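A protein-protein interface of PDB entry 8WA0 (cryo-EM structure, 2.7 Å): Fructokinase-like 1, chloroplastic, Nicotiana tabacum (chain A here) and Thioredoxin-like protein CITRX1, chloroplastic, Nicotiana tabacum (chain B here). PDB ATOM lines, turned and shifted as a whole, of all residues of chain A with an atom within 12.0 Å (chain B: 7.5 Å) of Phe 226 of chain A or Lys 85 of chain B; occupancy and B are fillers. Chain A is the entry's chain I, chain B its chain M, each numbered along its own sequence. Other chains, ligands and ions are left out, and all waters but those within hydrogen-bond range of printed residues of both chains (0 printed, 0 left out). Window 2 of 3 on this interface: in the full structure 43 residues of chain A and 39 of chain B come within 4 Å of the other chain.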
ATOM      1  N   MET A 222     -12.032  19.335 -17.375  1.00  0.00           N
ATOM      2  CA  MET A 222     -11.697  17.985 -16.990  1.00  0.00           C
ATOM      3  C   MET A 222     -12.691  17.481 -15.988  1.00  0.00           C
ATOM      4  O   MET A 222     -13.382  18.267 -15.366  1.00  0.00           O
ATOM      5  CB  MET A 222     -10.331  17.976 -16.344  1.00  0.00           C
ATOM      6  CG  MET A 222      -9.193  18.417 -17.243  1.00  0.00           C
ATOM      7  SD  MET A 222      -8.121  17.035 -17.656  1.00  0.00           S
ATOM      8  CE  MET A 222      -6.840  17.861 -18.582  1.00  0.00           C
ATOM      9  N   LYS A 223     -12.778  16.172 -15.821  1.00  0.00           N
ATOM     10  CA  LYS A 223     -13.665  15.612 -14.824  1.00  0.00           C
ATOM     11  C   LYS A 223     -12.864  14.808 -13.852  1.00  0.00           C
ATOM     12  O   LYS A 223     -12.210  13.857 -14.242  1.00  0.00           O
ATOM     13  CB  LYS A 223     -14.670  14.709 -15.497  1.00  0.00           C
ATOM     14  CG  LYS A 223     -15.844  14.322 -14.621  1.00  0.00           C
ATOM     15  CD  LYS A 223     -17.003  13.833 -15.472  1.00  0.00           C
ATOM     16  CE  LYS A 223     -17.427  14.902 -16.466  1.00  0.00           C
ATOM     17  NZ  LYS A 223     -18.587  14.473 -17.292  1.00  0.00           N
ATOM     18  N   ILE A 224     -12.939  15.145 -12.575  1.00  0.00           N
ATOM     19  CA  ILE A 224     -12.104  14.462 -11.603  1.00  0.00           C
ATOM     20  C   ILE A 224     -12.908  13.416 -10.905  1.00  0.00           C
ATOM     21  O   ILE A 224     -13.869  13.728 -10.219  1.00  0.00           O
ATOM     22  CB  ILE A 224     -11.529  15.418 -10.551  1.00  0.00           C
ATOM     23  N   LYS A 225     -12.514  12.165 -11.063  1.00  0.00           N
ATOM     24  CA  LYS A 225     -13.284  11.085 -10.492  1.00  0.00           C
ATOM     25  C   LYS A 225     -12.439  10.249  -9.592  1.00  0.00           C
ATOM     26  O   LYS A 225     -11.358   9.817  -9.971  1.00  0.00           O
ATOM     27  CB  LYS A 225     -13.839  10.207 -11.597  1.00  0.00           C
ATOM     28  CG  LYS A 225     -14.866  10.893 -12.479  1.00  0.00           C
ATOM     29  CD  LYS A 225     -15.099  10.098 -13.752  1.00  0.00           C
ATOM     30  CE  LYS A 225     -13.801   9.926 -14.523  1.00  0.00           C
ATOM     31  NZ  LYS A 225     -13.996   9.159 -15.783  1.00  0.00           N
ATOM     32  N   PHE A 226     -12.936   9.997  -8.392  1.00  0.00           N
ATOM     33  CA  PHE A 226     -12.204   9.142  -7.491  1.00  0.00           C
ATOM     34  C   PHE A 226     -12.929   7.830  -7.349  1.00  0.00           C
ATOM     35  O   PHE A 226     -14.050   7.794  -6.859  1.00  0.00           O
ATOM     36  CB  PHE A 226     -12.055   9.806  -6.124  1.00  0.00           C
ATOM     37  CG  PHE A 226     -10.784   9.445  -5.417  1.00  0.00           C
ATOM     38  CD1 PHE A 226     -10.682   8.267  -4.702  1.00  0.00           C
ATOM     39  CD2 PHE A 226      -9.687  10.282  -5.479  1.00  0.00           C
ATOM     40  CE1 PHE A 226      -9.509   7.932  -4.055  1.00  0.00           C
ATOM     41  CE2 PHE A 226      -8.511   9.955  -4.835  1.00  0.00           C
ATOM     42  CZ  PHE A 226      -8.420   8.776  -4.121  1.00  0.00           C
ATOM     43  N   GLU A 227     -12.301   6.746  -7.776  1.00  0.00           N
ATOM     44  CA  GLU A 227     -12.884   5.428  -7.582  1.00  0.00           C
ATOM     45  C   GLU A 227     -11.736   4.602  -7.057  1.00  0.00           C
ATOM     46  O   GLU A 227     -11.274   3.705  -7.765  1.00  0.00           O
ATOM     47  CB  GLU A 227     -13.377   4.862  -8.906  1.00  0.00           C
ATOM     48  N   ASP A 228     -11.243   4.934  -5.861  1.00  0.00           N
ATOM     49  CA  ASP A 228     -10.089   4.251  -5.249  1.00  0.00           C
ATOM     50  C   ASP A 228      -8.784   4.699  -5.907  1.00  0.00           C
ATOM     51  O   ASP A 228      -7.710   4.211  -5.563  1.00  0.00           O
ATOM     52  CB  ASP A 228     -10.243   2.722  -5.195  1.00  0.00           C
ATOM     53  N   GLY A 229      -8.874   5.640  -6.840  1.00  0.00           N
ATOM     54  CA  GLY A 229      -7.690   6.176  -7.484  1.00  0.00           C
ATOM     55  C   GLY A 229      -8.065   7.559  -7.963  1.00  0.00           C
ATOM     56  O   GLY A 229      -9.244   7.836  -8.159  1.00  0.00           O
ATOM     57  N   LYS A 230      -7.089   8.429  -8.172  1.00  0.00           N
ATOM     58  CA  LYS A 230      -7.402   9.734  -8.718  1.00  0.00           C
ATOM     59  C   LYS A 230      -7.408   9.607 -10.228  1.00  0.00           C
ATOM     60  O   LYS A 230      -6.399   9.257 -10.830  1.00  0.00           O
ATOM     61  CB  LYS A 230      -6.354  10.753  -8.291  1.00  0.00           C
ATOM     62  CG  LYS A 230      -6.540  12.130  -8.899  1.00  0.00           C
ATOM     63  CD  LYS A 230      -7.730  12.841  -8.286  1.00  0.00           C
ATOM     64  CE  LYS A 230      -7.454  13.192  -6.836  1.00  0.00           C
ATOM     65  NZ  LYS A 230      -8.656  13.759  -6.172  1.00  0.00           N
ATOM     66  N   MET A 231      -8.545   9.879 -10.848  1.00  0.00           N
ATOM     67  CA  MET A 231      -8.633   9.785 -12.288  1.00  0.00           C
ATOM     68  C   MET A 231      -9.115  11.082 -12.879  1.00  0.00           C
ATOM     69  O   MET A 231     -10.108  11.629 -12.428  1.00  0.00           O
ATOM     70  CB  MET A 231      -9.590   8.673 -12.680  1.00  0.00           C
ATOM     71  N   LYS A 232      -8.433  11.573 -13.897  1.00  0.00           N
ATOM     72  CA  LYS A 232      -8.890  12.767 -14.565  1.00  0.00           C
ATOM     73  C   LYS A 232      -9.189  12.401 -15.996  1.00  0.00           C
ATOM     74  O   LYS A 232      -8.415  11.697 -16.619  1.00  0.00           O
ATOM     75  CB  LYS A 232      -7.835  13.853 -14.493  1.00  0.00           C
ATOM     76  N   VAL A 233     -10.321  12.848 -16.516  1.00  0.00           N
ATOM     77  CA  VAL A 233     -10.683  12.570 -17.890  1.00  0.00           C
ATOM     78  C   VAL A 233     -11.044  13.878 -18.556  1.00  0.00           C
ATOM     79  O   VAL A 233     -11.467  14.797 -17.881  1.00  0.00           O
ATOM     80  CB  VAL A 233     -11.886  11.639 -17.943  1.00  0.00           C
ATOM     81  N   ALA B  77       0.008  15.119  -1.859  1.00  0.00           N
ATOM     82  CA  ALA B  77      -0.966  14.396  -2.620  1.00  0.00           C
ATOM     83  C   ALA B  77      -2.087  13.863  -1.801  1.00  0.00           C
ATOM     84  O   ALA B  77      -3.231  13.983  -2.195  1.00  0.00           O
ATOM     85  CB  ALA B  77      -0.300  13.259  -3.299  1.00  0.00           C
ATOM     86  N   LYS B  78      -1.800  13.297  -0.651  1.00  0.00           N
ATOM     87  CA  LYS B  78      -2.833  12.821   0.221  1.00  0.00           C
ATOM     88  C   LYS B  78      -3.754  13.905   0.710  1.00  0.00           C
ATOM     89  O   LYS B  78      -4.953  13.722   0.719  1.00  0.00           O
ATOM     90  CB  LYS B  78      -2.207  12.132   1.397  1.00  0.00           C
ATOM     91  CG  LYS B  78      -1.185  11.082   1.015  1.00  0.00           C
ATOM     92  CD  LYS B  78      -0.502  10.508   2.243  1.00  0.00           C
ATOM     93  CE  LYS B  78       0.615   9.554   1.852  1.00  0.00           C
ATOM     94  NZ  LYS B  78       1.649  10.232   1.022  1.00  0.00           N
ATOM     95  N   ASP B  79      -3.226  15.042   1.089  1.00  0.00           N
ATOM     96  CA  ASP B  79      -4.040  16.141   1.517  1.00  0.00           C
ATOM     97  C   ASP B  79      -4.916  16.682   0.448  1.00  0.00           C
ATOM     98  O   ASP B  79      -6.040  17.046   0.710  1.00  0.00           O
ATOM     99  CB  ASP B  79      -3.193  17.221   2.065  1.00  0.00           C
ATOM    100  CG  ASP B  79      -2.212  16.722   3.098  1.00  0.00           C
ATOM    101  OD1 ASP B  79      -2.491  15.689   3.741  1.00  0.00           O
ATOM    102  OD2 ASP B  79      -1.160  17.371   3.275  1.00  0.00           O
ATOM    103  N   ILE B  80      -4.426  16.749  -0.777  1.00  0.00           N
ATOM    104  CA  ILE B  80      -5.230  17.215  -1.883  1.00  0.00           C
ATOM    105  C   ILE B  80      -6.389  16.301  -2.103  1.00  0.00           C
ATOM    106  O   ILE B  80      -7.509  16.753  -2.309  1.00  0.00           O
ATOM    107  CB  ILE B  80      -4.411  17.483  -3.151  1.00  0.00           C
ATOM    108  CG1 ILE B  80      -3.620  18.771  -3.007  1.00  0.00           C
ATOM    109  CG2 ILE B  80      -5.307  17.613  -4.364  1.00  0.00           C
ATOM    110  CD1 ILE B  80      -4.494  19.983  -2.787  1.00  0.00           C
ATOM    111  N   GLN B  81      -6.166  15.019  -1.996  1.00  0.00           N
ATOM    112  CA  GLN B  81      -7.214  14.070  -2.171  1.00  0.00           C
ATOM    113  C   GLN B  81      -8.308  14.164  -1.149  1.00  0.00           C
ATOM    114  O   GLN B  81      -9.464  14.051  -1.504  1.00  0.00           O
ATOM    115  CB  GLN B  81      -6.621  12.699  -2.265  1.00  0.00           C
ATOM    116  CG  GLN B  81      -5.725  12.541  -3.476  1.00  0.00           C
ATOM    117  CD  GLN B  81      -4.950  11.248  -3.482  1.00  0.00           C
ATOM    118  OE1 GLN B  81      -5.032  10.454  -2.547  1.00  0.00           O
ATOM    119  NE2 GLN B  81      -4.183  11.029  -4.540  1.00  0.00           N
ATOM    120  N   GLU B  82      -7.992  14.403   0.099  1.00  0.00           N
ATOM    121  CA  GLU B  82      -9.028  14.591   1.085  1.00  0.00           C
ATOM    122  C   GLU B  82      -9.871  15.762   0.804  1.00  0.00           C
ATOM    123  O   GLU B  82     -11.075  15.693   0.930  1.00  0.00           O
ATOM    124  CB  GLU B  82      -8.453  14.774   2.459  1.00  0.00           C
ATOM    125  CG  GLU B  82      -7.534  13.651   2.894  1.00  0.00           C
ATOM    126  CD  GLU B  82      -6.446  14.128   3.834  1.00  0.00           C
ATOM    127  OE1 GLU B  82      -6.459  15.322   4.201  1.00  0.00           O
ATOM    128  OE2 GLU B  82      -5.575  13.312   4.202  1.00  0.00           O
ATOM    129  N   LEU B  83      -9.254  16.863   0.428  1.00  0.00           N
ATOM    130  CA  LEU B  83     -10.004  18.067   0.182  1.00  0.00           C
ATOM    131  C   LEU B  83     -10.957  17.840  -0.969  1.00  0.00           C
ATOM    132  O   LEU B  83     -12.091  18.297  -0.936  1.00  0.00           O
ATOM    133  CB  LEU B  83      -9.069  19.221  -0.130  1.00  0.00           C
ATOM    134  CG  LEU B  83      -8.160  19.744   0.973  1.00  0.00           C
ATOM    135  CD1 LEU B  83      -7.301  20.868   0.422  1.00  0.00           C
ATOM    136  CD2 LEU B  83      -8.990  20.236   2.142  1.00  0.00           C
ATOM    137  N   ILE B  84     -10.495  17.159  -2.008  1.00  0.00           N
ATOM    138  CA  ILE B  84     -11.353  16.882  -3.147  1.00  0.00           C
ATOM    139  C   ILE B  84     -12.505  15.968  -2.803  1.00  0.00           C
ATOM    140  O   ILE B  84     -13.635  16.228  -3.197  1.00  0.00           O
ATOM    141  CB  ILE B  84     -10.571  16.302  -4.324  1.00  0.00           C
ATOM    142  CG1 ILE B  84      -9.569  17.326  -4.828  1.00  0.00           C
ATOM    143  CG2 ILE B  84     -11.497  15.943  -5.471  1.00  0.00           C
ATOM    144  CD1 ILE B  84     -10.218  18.642  -5.173  1.00  0.00           C
ATOM    145  N   LYS B  85     -12.253  14.922  -2.031  1.00  0.00           N
ATOM    146  CA  LYS B  85     -13.319  13.969  -1.760  1.00  0.00           C
ATOM    147  C   LYS B  85     -14.281  14.514  -0.742  1.00  0.00           C
ATOM    148  O   LYS B  85     -15.469  14.243  -0.819  1.00  0.00           O
ATOM    149  CB  LYS B  85     -12.780  12.591  -1.380  1.00  0.00           C
ATOM    150  CG  LYS B  85     -12.053  12.506  -0.057  1.00  0.00           C
ATOM    151  CD  LYS B  85     -11.424  11.135   0.113  1.00  0.00           C
ATOM    152  CE  LYS B  85     -10.520  10.797  -1.061  1.00  0.00           C
ATOM    153  NZ  LYS B  85      -9.737   9.556  -0.812  1.00  0.00           N
ATOM    154  N   GLY B  86     -13.796  15.292   0.206  1.00  0.00           N
ATOM    155  CA  GLY B  86     -14.654  15.926   1.170  1.00  0.00           C
ATOM    156  C   GLY B  86     -15.416  17.096   0.622  1.00  0.00           C
ATOM    157  O   GLY B  86     -15.362  17.365  -0.571  1.00  0.00           O
ATOM    158  N   GLU B  87     -16.096  17.834   1.483  1.00  0.00           N
ATOM    159  CA  GLU B  87     -16.923  18.931   1.015  1.00  0.00           C
ATOM    160  C   GLU B  87     -16.228  20.256   1.133  1.00  0.00           C
ATOM    161  O   GLU B  87     -15.329  20.418   1.947  1.00  0.00           O
ATOM    162  CB  GLU B  87     -18.245  18.975   1.776  1.00  0.00           C
ATOM    163  CG  GLU B  87     -18.123  19.245   3.269  1.00  0.00           C
ATOM    164  CD  GLU B  87     -17.774  18.005   4.073  1.00  0.00           C
ATOM    165  OE1 GLU B  87     -18.033  16.885   3.587  1.00  0.00           O
ATOM    166  OE2 GLU B  87     -17.244  18.152   5.193  1.00  0.00           O
ATOM    167  N   ARG B  88     -16.635  21.208   0.309  1.00  0.00           N
ATOM    168  CA  ARG B  88     -16.031  22.521   0.339  1.00  0.00           C
ATOM    169  C   ARG B  88     -17.077  23.551   0.012  1.00  0.00           C
ATOM    170  O   ARG B  88     -18.083  23.234  -0.600  1.00  0.00           O
ATOM    171  CB  ARG B  88     -14.874  22.577  -0.645  1.00  0.00           C
ATOM    172  CG  ARG B  88     -15.251  22.173  -2.052  1.00  0.00           C
ATOM    173  CD  ARG B  88     -14.031  21.866  -2.894  1.00  0.00           C
ATOM    174  NE  ARG B  88     -14.433  21.229  -4.136  1.00  0.00           N
ATOM    175  CZ  ARG B  88     -14.571  19.919  -4.284  1.00  0.00           C
ATOM    176  NH1 ARG B  88     -14.321  19.107  -3.269  1.00  0.00           N
ATOM    177  NH2 ARG B  88     -14.952  19.421  -5.449  1.00  0.00           N
ATOM    178  N   PHE B 135       1.754  12.036  -9.063  1.00  0.00           N
ATOM    179  CA  PHE B 135       0.471  12.676  -9.003  1.00  0.00           C
ATOM    180  C   PHE B 135       0.286  13.590 -10.174  1.00  0.00           C
ATOM    181  O   PHE B 135      -0.791  13.638 -10.748  1.00  0.00           O
ATOM    182  CB  PHE B 135       0.308  13.420  -7.700  1.00  0.00           C
ATOM    183  CG  PHE B 135      -1.054  13.968  -7.449  1.00  0.00           C
ATOM    184  CD1 PHE B 135      -2.157  13.151  -7.456  1.00  0.00           C
ATOM    185  CD2 PHE B 135      -1.217  15.301  -7.149  1.00  0.00           C
ATOM    186  CE1 PHE B 135      -3.410  13.662  -7.207  1.00  0.00           C
ATOM    187  CE2 PHE B 135      -2.460  15.819  -6.894  1.00  0.00           C
ATOM    188  CZ  PHE B 135      -3.559  15.000  -6.923  1.00  0.00           C
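The guanidinium group of Arg 88 of chain B is in hydrogen-bond range of the backbone carbonyl oxygen of Ile 84 of chain B, 3.0 Å away.
Phe 226 of chain A touches Lys 85 of chain B (CE1 to NZ, 3.6 Å).
CG of Gln 81 of chain B touches CE of Lys 230 of chain A, at 3.8 Å.
Ile 84 of chain B touches Lys 230 of chain A.
CG of Lys 230 of chain A touches CE1 of Phe 135 of chain B (3.9 Å).
Of the printed residues of chain B, Phe 226 of chain A touches Lys 85 (3.6 Å).
Lys 85 of chain B touches one residue of chain A.
Printed residues of chain A within 4 Å of Gln 81 of chain B: Lys 230 (3.8 Å).
No residue of chain A comes within 4 Å of Glu 82 of chain B.
Printed residues of chain A within 4 Å of Ile 84 of chain B: Lys 230.
No residue of chain A comes within 4 Å of Glu 87 of chain B.
Printed residues of chain B within 4 Å of Lys 230 of chain A: Gln 81 (3.8 Å), Ile 84 (3.7 Å) and Phe 135 (3.9 Å).
Printed residues of chain A within 4 Å of Phe 135 of chain B: Lys 230 (3.9 Å).
The nearest residue of chain B that does not touch Phe 226 of chain A is Gln 81 of chain B (4.02 Å).
The nearest residue of chain A that does not touch Lys 85 of chain B is Lys 230 of chain A (5.6 Å).
Of the 13 printed residues of chain B, 4 touch a printed residue of chain A.
Hydrophobic or aromatic side chains of chain A within 4 Å of the printed part of chain B: Phe 226.
Along chain A the printed residues that touch a printed residue of chain B span positions 226 to 230.
Among the printed residues, 4 pairs touch across the chains.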
